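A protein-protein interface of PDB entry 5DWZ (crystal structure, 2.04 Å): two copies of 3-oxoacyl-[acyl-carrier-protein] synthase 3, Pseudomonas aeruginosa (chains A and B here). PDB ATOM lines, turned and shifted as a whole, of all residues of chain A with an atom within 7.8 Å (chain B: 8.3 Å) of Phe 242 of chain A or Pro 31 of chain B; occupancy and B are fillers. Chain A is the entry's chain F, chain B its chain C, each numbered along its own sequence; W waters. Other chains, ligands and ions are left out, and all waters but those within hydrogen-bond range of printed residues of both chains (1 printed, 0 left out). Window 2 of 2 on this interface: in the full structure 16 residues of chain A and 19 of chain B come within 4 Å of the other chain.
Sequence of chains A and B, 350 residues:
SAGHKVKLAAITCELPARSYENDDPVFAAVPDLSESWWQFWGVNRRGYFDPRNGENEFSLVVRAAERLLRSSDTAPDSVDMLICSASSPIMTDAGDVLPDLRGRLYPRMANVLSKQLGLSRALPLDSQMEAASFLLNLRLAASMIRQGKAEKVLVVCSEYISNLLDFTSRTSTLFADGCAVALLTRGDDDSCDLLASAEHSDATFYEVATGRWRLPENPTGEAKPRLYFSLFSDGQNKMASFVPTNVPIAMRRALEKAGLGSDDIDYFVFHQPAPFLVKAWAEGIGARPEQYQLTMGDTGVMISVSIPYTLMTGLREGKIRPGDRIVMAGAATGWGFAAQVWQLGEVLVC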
ATOM      1  N   ASP A 202      -7.160   7.458  39.881  1.00  0.00           N
ATOM      2  CA  ASP A 202      -6.935   6.120  39.345  1.00  0.00           C
ATOM      3  C   ASP A 202      -5.849   5.490  40.146  1.00  0.00           C
ATOM      4  O   ASP A 202      -4.729   5.964  40.141  1.00  0.00           O
ATOM      5  CB  ASP A 202      -6.558   6.183  37.849  1.00  0.00           C
ATOM      6  CG  ASP A 202      -6.559   4.820  37.170  1.00  0.00           C
ATOM      7  OD1 ASP A 202      -6.215   3.814  37.801  1.00  0.00           O
ATOM      8  OD2 ASP A 202      -6.950   4.752  35.994  1.00  0.00           O
ATOM      9  N   PHE A 205      -1.828   2.248  39.459  1.00  0.00           N
ATOM     10  CA  PHE A 205      -0.431   2.393  39.766  1.00  0.00           C
ATOM     11  C   PHE A 205      -0.148   2.998  41.128  1.00  0.00           C
ATOM     12  O   PHE A 205       0.904   3.574  41.344  1.00  0.00           O
ATOM     13  CB  PHE A 205       0.293   3.204  38.660  1.00  0.00           C
ATOM     14  CG  PHE A 205       0.296   2.514  37.330  1.00  0.00           C
ATOM     15  CD1 PHE A 205       1.000   1.304  37.159  1.00  0.00           C
ATOM     16  CD2 PHE A 205      -0.449   3.006  36.255  1.00  0.00           C
ATOM     17  CE1 PHE A 205       0.968   0.637  35.925  1.00  0.00           C
ATOM     18  CE2 PHE A 205      -0.473   2.343  35.032  1.00  0.00           C
ATOM     19  CZ  PHE A 205       0.232   1.155  34.871  1.00  0.00           C
ATOM     20  N   GLY A 235       2.730  -4.825  30.769  1.00  0.00           N
ATOM     21  CA  GLY A 235       2.191  -3.953  29.720  1.00  0.00           C
ATOM     22  C   GLY A 235       0.671  -4.097  29.577  1.00  0.00           C
ATOM     23  O   GLY A 235       0.041  -3.230  29.003  1.00  0.00           O
ATOM     24  N   GLN A 236       0.085  -5.184  30.086  1.00  0.00           N
ATOM     25  CA  GLN A 236      -1.330  -5.518  29.853  1.00  0.00           C
ATOM     26  C   GLN A 236      -2.314  -4.871  30.792  1.00  0.00           C
ATOM     27  O   GLN A 236      -3.502  -4.848  30.492  1.00  0.00           O
ATOM     28  CB  GLN A 236      -1.553  -7.030  29.904  1.00  0.00           C
ATOM     29  CG  GLN A 236      -0.626  -7.834  29.005  1.00  0.00           C
ATOM     30  CD  GLN A 236      -1.038  -9.309  28.929  1.00  0.00           C
ATOM     31  OE1 GLN A 236      -0.363 -10.172  29.494  1.00  0.00           O
ATOM     32  NE2 GLN A 236      -2.133  -9.604  28.217  1.00  0.00           N
ATOM     33  N   ASN A 237      -1.831  -4.381  31.928  1.00  0.00           N
ATOM     34  CA  ASN A 237      -2.687  -3.719  32.916  1.00  0.00           C
ATOM     35  C   ASN A 237      -2.463  -2.203  32.983  1.00  0.00           C
ATOM     36  O   ASN A 237      -1.766  -1.682  33.851  1.00  0.00           O
ATOM     37  CB  ASN A 237      -2.607  -4.395  34.284  1.00  0.00           C
ATOM     38  CG  ASN A 237      -3.714  -3.919  35.227  1.00  0.00           C
ATOM     39  OD1 ASN A 237      -4.734  -3.412  34.768  1.00  0.00           O
ATOM     40  ND2 ASN A 237      -3.507  -4.039  36.543  1.00  0.00           N
ATOM     41  N   LYS A 238      -3.123  -1.507  32.069  1.00  0.00           N
ATOM     42  CA  LYS A 238      -3.002  -0.074  31.943  1.00  0.00           C
ATOM     43  C   LYS A 238      -4.164   0.643  32.632  1.00  0.00           C
ATOM     44  O   LYS A 238      -5.165   0.035  32.958  1.00  0.00           O
ATOM     45  CB  LYS A 238      -2.974   0.286  30.466  1.00  0.00           C
ATOM     46  CG  LYS A 238      -1.908  -0.460  29.637  1.00  0.00           C
ATOM     47  CD  LYS A 238      -1.453   0.422  28.446  1.00  0.00           C
ATOM     48  CE  LYS A 238      -1.231  -0.309  27.123  1.00  0.00           C
ATOM     49  NZ  LYS A 238      -0.223  -1.386  27.253  1.00  0.00           N
ATOM     50  N   MET A 239      -4.009   1.938  32.842  1.00  0.00           N
ATOM     51  CA  MET A 239      -5.154   2.792  33.249  1.00  0.00           C
ATOM     52  C   MET A 239      -6.197   2.865  32.123  1.00  0.00           C
ATOM     53  O   MET A 239      -5.892   2.658  30.927  1.00  0.00           O
ATOM     54  CB  MET A 239      -4.698   4.184  33.583  1.00  0.00           C
ATOM     55  CG  MET A 239      -3.775   4.253  34.771  1.00  0.00           C
ATOM     56  SD  MET A 239      -3.463   5.923  35.334  1.00  0.00           S
ATOM     57  CE  MET A 239      -2.227   6.435  34.170  1.00  0.00           C
ATOM     58  N   ALA A 240      -7.439   3.103  32.520  1.00  0.00           N
ATOM     59  CA  ALA A 240      -8.569   3.262  31.569  1.00  0.00           C
ATOM     60  C   ALA A 240      -8.289   4.413  30.600  1.00  0.00           C
ATOM     61  O   ALA A 240      -8.589   4.330  29.424  1.00  0.00           O
ATOM     62  CB  ALA A 240      -9.878   3.497  32.307  1.00  0.00           C
ATOM     63  N   SER A 241      -7.669   5.464  31.104  1.00  0.00           N
ATOM     64  CA  SER A 241      -7.145   6.521  30.278  1.00  0.00           C
ATOM     65  C   SER A 241      -5.629   6.509  30.367  1.00  0.00           C
ATOM     66  O   SER A 241      -5.055   6.655  31.466  1.00  0.00           O
ATOM     67  CB  SER A 241      -7.634   7.894  30.745  1.00  0.00           C
ATOM     68  OG  SER A 241      -9.027   7.999  30.620  1.00  0.00           O
ATOM     69  N   PHE A 242      -4.980   6.383  29.209  1.00  0.00           N
ATOM     70  CA  PHE A 242      -3.515   6.200  29.191  1.00  0.00           C
ATOM     71  C   PHE A 242      -2.795   7.488  29.509  1.00  0.00           C
ATOM     72  O   PHE A 242      -3.270   8.575  29.211  1.00  0.00           O
ATOM     73  CB  PHE A 242      -2.992   5.673  27.840  1.00  0.00           C
ATOM     74  CG  PHE A 242      -3.720   4.463  27.313  1.00  0.00           C
ATOM     75  CD1 PHE A 242      -4.003   3.378  28.137  1.00  0.00           C
ATOM     76  CD2 PHE A 242      -4.072   4.395  25.960  1.00  0.00           C
ATOM     77  CE1 PHE A 242      -4.678   2.270  27.640  1.00  0.00           C
ATOM     78  CE2 PHE A 242      -4.737   3.286  25.453  1.00  0.00           C
ATOM     79  CZ  PHE A 242      -5.020   2.213  26.292  1.00  0.00           C
ATOM     80  N   VAL A 243      -1.592   7.382  30.025  1.00  0.00           N
ATOM     81  CA  VAL A 243      -0.767   8.524  30.223  1.00  0.00           C
ATOM     82  C   VAL A 243      -0.486   8.913  28.786  1.00  0.00           C
ATOM     83  O   VAL A 243      -0.381   8.051  27.984  1.00  0.00           O
ATOM     84  CB  VAL A 243       0.547   8.086  30.833  1.00  0.00           C
ATOM     85  CG1 VAL A 243       1.540   9.204  30.850  1.00  0.00           C
ATOM     86  CG2 VAL A 243       0.346   7.512  32.208  1.00  0.00           C
ATOM     87  N   PRO A 244      -0.348  10.229  28.382  1.00  0.00           N
ATOM     88  CA  PRO A 244      -0.499  11.278  29.383  1.00  0.00           C
ATOM     89  C   PRO A 244      -1.818  12.052  29.335  1.00  0.00           C
ATOM     90  O   PRO A 244      -1.857  13.231  29.528  1.00  0.00           O
ATOM     91  CB  PRO A 244       0.667  12.191  29.057  1.00  0.00           C
ATOM     92  CG  PRO A 244       0.760  12.161  27.599  1.00  0.00           C
ATOM     93  CD  PRO A 244       0.036  10.960  27.099  1.00  0.00           C
ATOM     94  N   THR A 245      -2.882  11.361  29.044  1.00  0.00           N
ATOM     95  CA  THR A 245      -4.160  11.973  28.918  1.00  0.00           C
ATOM     96  C   THR A 245      -5.052  12.221  30.134  1.00  0.00           C
ATOM     97  O   THR A 245      -6.138  12.691  29.971  1.00  0.00           O
ATOM     98  CB  THR A 245      -4.968  11.141  27.942  1.00  0.00           C
ATOM     99  OG1 THR A 245      -5.460   9.995  28.594  1.00  0.00           O
ATOM    100  CG2 THR A 245      -4.122  10.701  26.772  1.00  0.00           C
ATOM    101  N   ASN A 246      -4.605  11.900  31.334  1.00  0.00           N
ATOM    102  CA  ASN A 246      -5.500  12.026  32.521  1.00  0.00           C
ATOM    103  C   ASN A 246      -5.694  13.483  32.888  1.00  0.00           C
ATOM    104  O   ASN A 246      -6.806  13.917  33.084  1.00  0.00           O
ATOM    105  CB  ASN A 246      -5.028  11.238  33.701  1.00  0.00           C
ATOM    106  CG  ASN A 246      -5.296   9.782  33.536  1.00  0.00           C
ATOM    107  OD1 ASN A 246      -6.431   9.301  33.752  1.00  0.00           O
ATOM    108  ND2 ASN A 246      -4.280   9.055  33.053  1.00  0.00           N
ATOM    109  N   VAL A 247      -4.604  14.218  32.876  1.00  0.00           N
ATOM    110  CA  VAL A 247      -4.643  15.660  33.105  1.00  0.00           C
ATOM    111  C   VAL A 247      -5.450  16.390  32.001  1.00  0.00           C
ATOM    112  O   VAL A 247      -6.366  17.133  32.323  1.00  0.00           O
ATOM    113  CB  VAL A 247      -3.279  16.279  33.388  1.00  0.00           C
ATOM    114  CG1 VAL A 247      -3.325  17.802  33.333  1.00  0.00           C
ATOM    115  CG2 VAL A 247      -2.826  15.843  34.771  1.00  0.00           C
ATOM    116  N   PRO A 248      -5.153  16.148  30.704  1.00  0.00           N
ATOM    117  CA  PRO A 248      -6.066  16.659  29.652  1.00  0.00           C
ATOM    118  C   PRO A 248      -7.532  16.277  29.791  1.00  0.00           C
ATOM    119  O   PRO A 248      -8.409  17.086  29.483  1.00  0.00           O
ATOM    120  CB  PRO A 248      -5.482  16.061  28.363  1.00  0.00           C
ATOM    121  CG  PRO A 248      -4.032  15.984  28.653  1.00  0.00           C
ATOM    122  CD  PRO A 248      -3.900  15.658  30.124  1.00  0.00           C
ATOM    123  N   ILE A 249      -7.803  15.048  30.191  1.00  0.00           N
ATOM    124  CA  ILE A 249      -9.206  14.601  30.385  1.00  0.00           C
ATOM    125  C   ILE A 249      -9.900  15.421  31.490  1.00  0.00           C
ATOM    126  O   ILE A 249     -11.040  15.862  31.335  1.00  0.00           O
ATOM    127  CB  ILE A 249      -9.327  13.095  30.642  1.00  0.00           C
ATOM    128  CG1 ILE A 249      -9.147  12.363  29.310  1.00  0.00           C
ATOM    129  CG2 ILE A 249     -10.697  12.723  31.216  1.00  0.00           C
ATOM    130  CD1 ILE A 249      -8.943  10.877  29.422  1.00  0.00           C
ATOM    131  N   PHE B  27       0.413   0.542  14.494  1.00  0.00           N
ATOM    132  CA  PHE B  27       0.438   1.115  15.854  1.00  0.00           C
ATOM    133  C   PHE B  27      -0.902   1.718  16.388  1.00  0.00           C
ATOM    134  O   PHE B  27      -0.920   2.448  17.390  1.00  0.00           O
ATOM    135  CB  PHE B  27       1.538   2.197  15.943  1.00  0.00           C
ATOM    136  CG  PHE B  27       2.922   1.702  15.595  1.00  0.00           C
ATOM    137  CD1 PHE B  27       3.457   0.546  16.214  1.00  0.00           C
ATOM    138  CD2 PHE B  27       3.710   2.393  14.682  1.00  0.00           C
ATOM    139  CE1 PHE B  27       4.724   0.102  15.889  1.00  0.00           C
ATOM    140  CE2 PHE B  27       5.005   1.965  14.384  1.00  0.00           C
ATOM    141  CZ  PHE B  27       5.508   0.820  14.993  1.00  0.00           C
ATOM    142  N   ALA B  28      -2.002   1.389  15.740  1.00  0.00           N
ATOM    143  CA  ALA B  28      -3.315   1.981  16.065  1.00  0.00           C
ATOM    144  C   ALA B  28      -3.759   1.741  17.534  1.00  0.00           C
ATOM    145  O   ALA B  28      -4.293   2.647  18.159  1.00  0.00           O
ATOM    146  CB  ALA B  28      -4.389   1.472  15.110  1.00  0.00           C
ATOM    147  N   ALA B  29      -3.529   0.529  18.025  1.00  0.00           N
ATOM    148  CA  ALA B  29      -3.826   0.125  19.401  1.00  0.00           C
ATOM    149  C   ALA B  29      -2.756   0.513  20.429  1.00  0.00           C
ATOM    150  O   ALA B  29      -2.917   0.244  21.606  1.00  0.00           O
ATOM    151  CB  ALA B  29      -4.074  -1.364  19.457  1.00  0.00           C
ATOM    152  N   VAL B  30      -1.688   1.171  19.986  1.00  0.00           N
ATOM    153  CA  VAL B  30      -0.659   1.665  20.892  1.00  0.00           C
ATOM    154  C   VAL B  30      -1.150   2.980  21.474  1.00  0.00           C
ATOM    155  O   VAL B  30      -1.660   3.808  20.733  1.00  0.00           O
ATOM    156  CB  VAL B  30       0.704   1.892  20.193  1.00  0.00           C
ATOM    157  CG1 VAL B  30       1.732   2.426  21.170  1.00  0.00           C
ATOM    158  CG2 VAL B  30       1.208   0.582  19.595  1.00  0.00           C
ATOM    159  N   PRO B  31      -0.966   3.201  22.795  1.00  0.00           N
ATOM    160  CA  PRO B  31      -1.285   4.524  23.299  1.00  0.00           C
ATOM    161  C   PRO B  31      -0.630   5.633  22.519  1.00  0.00           C
ATOM    162  O   PRO B  31       0.530   5.523  22.093  1.00  0.00           O
ATOM    163  CB  PRO B  31      -0.729   4.517  24.720  1.00  0.00           C
ATOM    164  CG  PRO B  31      -0.795   3.086  25.129  1.00  0.00           C
ATOM    165  CD  PRO B  31      -0.511   2.310  23.870  1.00  0.00           C
ATOM    166  N   ASP B  32      -1.385   6.711  22.348  1.00  0.00           N
ATOM    167  CA  ASP B  32      -0.920   7.852  21.600  1.00  0.00           C
ATOM    168  C   ASP B  32       0.400   8.337  22.159  1.00  0.00           C
ATOM    169  O   ASP B  32       0.595   8.426  23.355  1.00  0.00           O
ATOM    170  CB  ASP B  32      -1.936   9.011  21.617  1.00  0.00           C
ATOM    171  CG  ASP B  32      -3.203   8.713  20.822  1.00  0.00           C
ATOM    172  OD1 ASP B  32      -3.255   7.785  19.976  1.00  0.00           O
ATOM    173  OD2 ASP B  32      -4.184   9.431  21.053  1.00  0.00           O
ATOM    174  N   LEU B  33       1.279   8.687  21.241  1.00  0.00           N
ATOM    175  CA  LEU B  33       2.637   9.139  21.538  1.00  0.00           C
ATOM    176  C   LEU B  33       2.890  10.427  20.781  1.00  0.00           C
ATOM    177  O   LEU B  33       2.363  10.661  19.694  1.00  0.00           O
ATOM    178  CB  LEU B  33       3.703   8.101  21.076  1.00  0.00           C
ATOM    179  CG  LEU B  33       4.186   6.879  21.893  1.00  0.00           C
ATOM    180  CD1 LEU B  33       3.568   6.750  23.261  1.00  0.00           C
ATOM    181  CD2 LEU B  33       4.331   5.626  21.082  1.00  0.00           C
ATOM    182  N   SER B  34       3.793  11.205  21.318  1.00  0.00           N
ATOM    183  CA  SER B  34       4.153  12.517  20.775  1.00  0.00           C
ATOM    184  C   SER B  34       5.575  12.567  20.245  1.00  0.00           C
ATOM    185  O   SER B  34       6.343  11.606  20.345  1.00  0.00           O
ATOM    186  CB  SER B  34       4.054  13.522  21.898  1.00  0.00           C
ATOM    187  OG  SER B  34       5.049  13.241  22.861  1.00  0.00           O
ATOM    188  N   TRP B  37       8.404  11.372  22.641  1.00  0.00           N
ATOM    189  CA  TRP B  37       8.728   9.931  22.614  1.00  0.00           C
ATOM    190  C   TRP B  37       9.681   9.604  21.471  1.00  0.00           C
ATOM    191  O   TRP B  37      10.722   8.992  21.675  1.00  0.00           O
ATOM    192  CB  TRP B  37       7.456   9.093  22.470  1.00  0.00           C
ATOM    193  CG  TRP B  37       7.667   7.576  22.399  1.00  0.00           C
ATOM    194  CD1 TRP B  37       7.759   6.830  21.291  1.00  0.00           C
ATOM    195  CD2 TRP B  37       7.789   6.679  23.504  1.00  0.00           C
ATOM    196  NE1 TRP B  37       7.920   5.515  21.613  1.00  0.00           N
ATOM    197  CE2 TRP B  37       7.950   5.388  22.976  1.00  0.00           C
ATOM    198  CE3 TRP B  37       7.785   6.839  24.894  1.00  0.00           C
ATOM    199  CZ2 TRP B  37       8.104   4.262  23.781  1.00  0.00           C
ATOM    200  CZ3 TRP B  37       7.938   5.697  25.701  1.00  0.00           C
ATOM    201  CH2 TRP B  37       8.103   4.436  25.136  1.00  0.00           C
ATOM    202  N   TRP B  38       9.315  10.058  20.286  1.00  0.00           N
ATOM    203  CA  TRP B  38      10.081   9.810  19.072  1.00  0.00           C
ATOM    204  C   TRP B  38      11.476  10.429  19.141  1.00  0.00           C
ATOM    205  O   TRP B  38      12.429   9.787  18.695  1.00  0.00           O
ATOM    206  CB  TRP B  38       9.336  10.238  17.791  1.00  0.00           C
ATOM    207  CG  TRP B  38       7.965   9.662  17.708  1.00  0.00           C
ATOM    208  CD1 TRP B  38       6.793  10.357  17.656  1.00  0.00           C
ATOM    209  CD2 TRP B  38       7.610   8.278  17.696  1.00  0.00           C
ATOM    210  NE1 TRP B  38       5.726   9.492  17.608  1.00  0.00           N
ATOM    211  CE2 TRP B  38       6.194   8.206  17.617  1.00  0.00           C
ATOM    212  CE3 TRP B  38       8.349   7.086  17.754  1.00  0.00           C
ATOM    213  CZ2 TRP B  38       5.496   6.971  17.592  1.00  0.00           C
ATOM    214  CZ3 TRP B  38       7.670   5.883  17.708  1.00  0.00           C
ATOM    215  CH2 TRP B  38       6.257   5.823  17.613  1.00  0.00           C
ATOM    216  N   ASP B 166       4.059  -6.753  21.293  1.00  0.00           N
ATOM    217  CA  ASP B 166       2.674  -6.470  21.650  1.00  0.00           C
ATOM    218  C   ASP B 166       2.351  -5.092  21.071  1.00  0.00           C
ATOM    219  O   ASP B 166       2.730  -4.071  21.617  1.00  0.00           O
ATOM    220  CB  ASP B 166       2.538  -6.492  23.172  1.00  0.00           C
ATOM    221  CG  ASP B 166       1.103  -6.270  23.655  1.00  0.00           C
ATOM    222  OD1 ASP B 166       0.218  -5.859  22.894  1.00  0.00           O
ATOM    223  OD2 ASP B 166       0.869  -6.536  24.833  1.00  0.00           O
ATOM    224  N   PHE B 167       1.628  -5.094  19.957  1.00  0.00           N
ATOM    225  CA  PHE B 167       1.225  -3.860  19.299  1.00  0.00           C
ATOM    226  C   PHE B 167       0.093  -3.083  20.031  1.00  0.00           C
ATOM    227  O   PHE B 167      -0.474  -2.152  19.471  1.00  0.00           O
ATOM    228  CB  PHE B 167       0.944  -4.129  17.819  1.00  0.00           C
ATOM    229  CG  PHE B 167       2.197  -4.476  17.036  1.00  0.00           C
ATOM    230  CD1 PHE B 167       3.043  -3.462  16.527  1.00  0.00           C
ATOM    231  CD2 PHE B 167       2.595  -5.804  16.905  1.00  0.00           C
ATOM    232  CE1 PHE B 167       4.217  -3.777  15.854  1.00  0.00           C
ATOM    233  CE2 PHE B 167       3.768  -6.131  16.218  1.00  0.00           C
ATOM    234  CZ  PHE B 167       4.583  -5.111  15.697  1.00  0.00           C
ATOM    235  N   THR B 168      -0.212  -3.473  21.272  1.00  0.00           N
ATOM    236  CA  THR B 168      -0.998  -2.602  22.213  1.00  0.00           C
ATOM    237  C   THR B 168      -0.102  -1.831  23.182  1.00  0.00           C
ATOM    238  O   THR B 168      -0.563  -0.997  23.947  1.00  0.00           O
ATOM    239  CB  THR B 168      -2.060  -3.363  23.041  1.00  0.00           C
ATOM    240  OG1 THR B 168      -1.419  -4.221  23.989  1.00  0.00           O
ATOM    241  CG2 THR B 168      -2.980  -4.168  22.128  1.00  0.00           C
ATOM    242  N   SER B 169       1.191  -2.087  23.090  1.00  0.00           N
ATOM    243  CA  SER B 169       2.146  -1.480  23.977  1.00  0.00           C
ATOM    244  C   SER B 169       3.131  -0.526  23.294  1.00  0.00           C
ATOM    245  O   SER B 169       3.556  -0.735  22.148  1.00  0.00           O
ATOM    246  CB  SER B 169       2.833  -2.559  24.802  1.00  0.00           C
ATOM    247  OG  SER B 169       1.836  -3.046  25.717  1.00  0.00           O
ATOM    248  N   ARG B 170       3.550   0.463  24.052  1.00  0.00           N
ATOM    249  CA  ARG B 170       4.481   1.439  23.601  1.00  0.00           C
ATOM    250  C   ARG B 170       5.796   0.798  23.201  1.00  0.00           C
ATOM    251  O   ARG B 170       6.447   1.301  22.348  1.00  0.00           O
ATOM    252  CB  ARG B 170       4.744   2.490  24.671  1.00  0.00           C
ATOM    253  CG  ARG B 170       3.582   3.385  24.997  1.00  0.00           C
ATOM    254  CD  ARG B 170       3.898   4.259  26.173  1.00  0.00           C
ATOM    255  NE  ARG B 170       2.757   5.002  26.671  1.00  0.00           N
ATOM    256  CZ  ARG B 170       1.823   4.547  27.491  1.00  0.00           C
ATOM    257  NH1 ARG B 170       1.821   3.322  27.922  1.00  0.00           N
ATOM    258  NH2 ARG B 170       0.869   5.337  27.866  1.00  0.00           N
ATOM    259  N   THR B 171       6.166  -0.290  23.859  1.00  0.00           N
ATOM    260  CA  THR B 171       7.450  -0.993  23.614  1.00  0.00           C
ATOM    261  C   THR B 171       7.595  -1.463  22.178  1.00  0.00           C
ATOM    262  O   THR B 171       8.719  -1.518  21.665  1.00  0.00           O
ATOM    263  CB  THR B 171       7.695  -2.195  24.563  1.00  0.00           C
ATOM    264  OG1 THR B 171       6.539  -3.017  24.584  1.00  0.00           O
ATOM    265  CG2 THR B 171       8.002  -1.731  25.927  1.00  0.00           C
ATOM    266  N   SER B 172       6.464  -1.791  21.569  1.00  0.00           N
ATOM    267  CA  SER B 172       6.375  -2.221  20.166  1.00  0.00           C
ATOM    268  C   SER B 172       6.899  -1.216  19.147  1.00  0.00           C
ATOM    269  O   SER B 172       7.326  -1.623  18.111  1.00  0.00           O
ATOM    270  CB  SER B 172       4.967  -2.673  19.806  1.00  0.00           C
ATOM    271  OG  SER B 172       4.082  -1.609  19.652  1.00  0.00           O
ATOM    272  N   THR B 173       6.938   0.060  19.514  1.00  0.00           N
ATOM    273  CA  THR B 173       7.454   1.135  18.634  1.00  0.00           C
ATOM    274  C   THR B 173       8.981   1.258  18.575  1.00  0.00           C
ATOM    275  O   THR B 173       9.530   1.971  17.764  1.00  0.00           O
ATOM    276  CB  THR B 173       6.873   2.516  19.057  1.00  0.00           C
ATOM    277  OG1 THR B 173       7.357   2.924  20.353  1.00  0.00           O
ATOM    278  CG2 THR B 173       5.359   2.470  19.056  1.00  0.00           C
HETATM  279  O   HOH W   1      -1.685   7.773  25.338  1.00  0.00           O
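O of Thr 168 of chain B sits close to NZ of Lys 238 of chain A (3.3 Å). The side-chain hydroxyl of Ser 169 of chain B sits at hydrogen-bond distance from the side-chain amino group of Lys 238 of chain A (3.1 Å). The guanidinium group of Arg 170 of chain B is in hydrogen-bond range of the backbone carbonyl oxygen of Val 243 of chain A (3.0 Å).
The side-chain hydroxyl (OG) of Ser 172 of chain B sits at hydrogen-bond distance from the backbone carbonyl oxygen (O) of Ser 169 of chain B, at 2.7 Å. The side-chain hydroxyl of Thr 245 of chain A is in hydrogen-bond range of the backbone carbonyl oxygen of Phe 242 of chain A. O of Arg 170 of chain B is in hydrogen-bond range of OG1 of Thr 173 of chain B (2.7 Å). The side-chain carboxylate (OD1) of Asp 166 of chain B lies within hydrogen-bond range of the side-chain hydroxyl (OG1) of Thr 168 of chain B, 2.6 Å away. O of Gly 235 of chain A lies within hydrogen-bond range of NZ of Lys 238 of chain A, at 2.6 Å.
Among the printed residues, merely in contact across the chains: Gly 235 of chain A with Ser 169 of chain B (3.7 Å), Lys 238 of chain A with Pro 31 of chain B (3.96 Å), Phe 242 of chain A with Pro 31 of chain B (3.6 Å) and Phe 242 of chain A with Arg 170 of chain B (3.9 Å).
Of the printed residues of chain B, Gly 235 of chain A touches Ser 169 (3.7 Å). Gln 236 of chain A touches none of the printed residues of chain B. Of chain B, only Pro 31 (3.6 Å) and Arg 170 (3.9 Å) come within 4 Å of Phe 242 of chain A. Printed residues of chain B within 4 Å of Val 243 of chain A: Arg 170 (3.0 Å). Of chain A, only Lys 238 and Phe 242 come within 4 Å of Pro 31 of chain B. Of the printed residues of chain A, Thr 168 of chain B touches Lys 238 (3.3 Å). The nearest residue of chain A that does not touch Pro 31 of chain B is Val 243 of chain A (4.8 Å).
Printed residues of chain A that touch a printed residue of chain B: Gly 235, Lys 238, Phe 242 and Val 243. Of the 18 printed residues of chain B, 4 touch a printed residue of chain A. Hydrophobic or aromatic side chains of chain B within 4 Å of the printed part of chain A: Pro 31.
No position is printed for both chains.
Water W1 lies within hydrogen-bond range of O of Val 243 of chain A (3.0 Å) and O of Asp 32 of chain B (3.1 Å).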
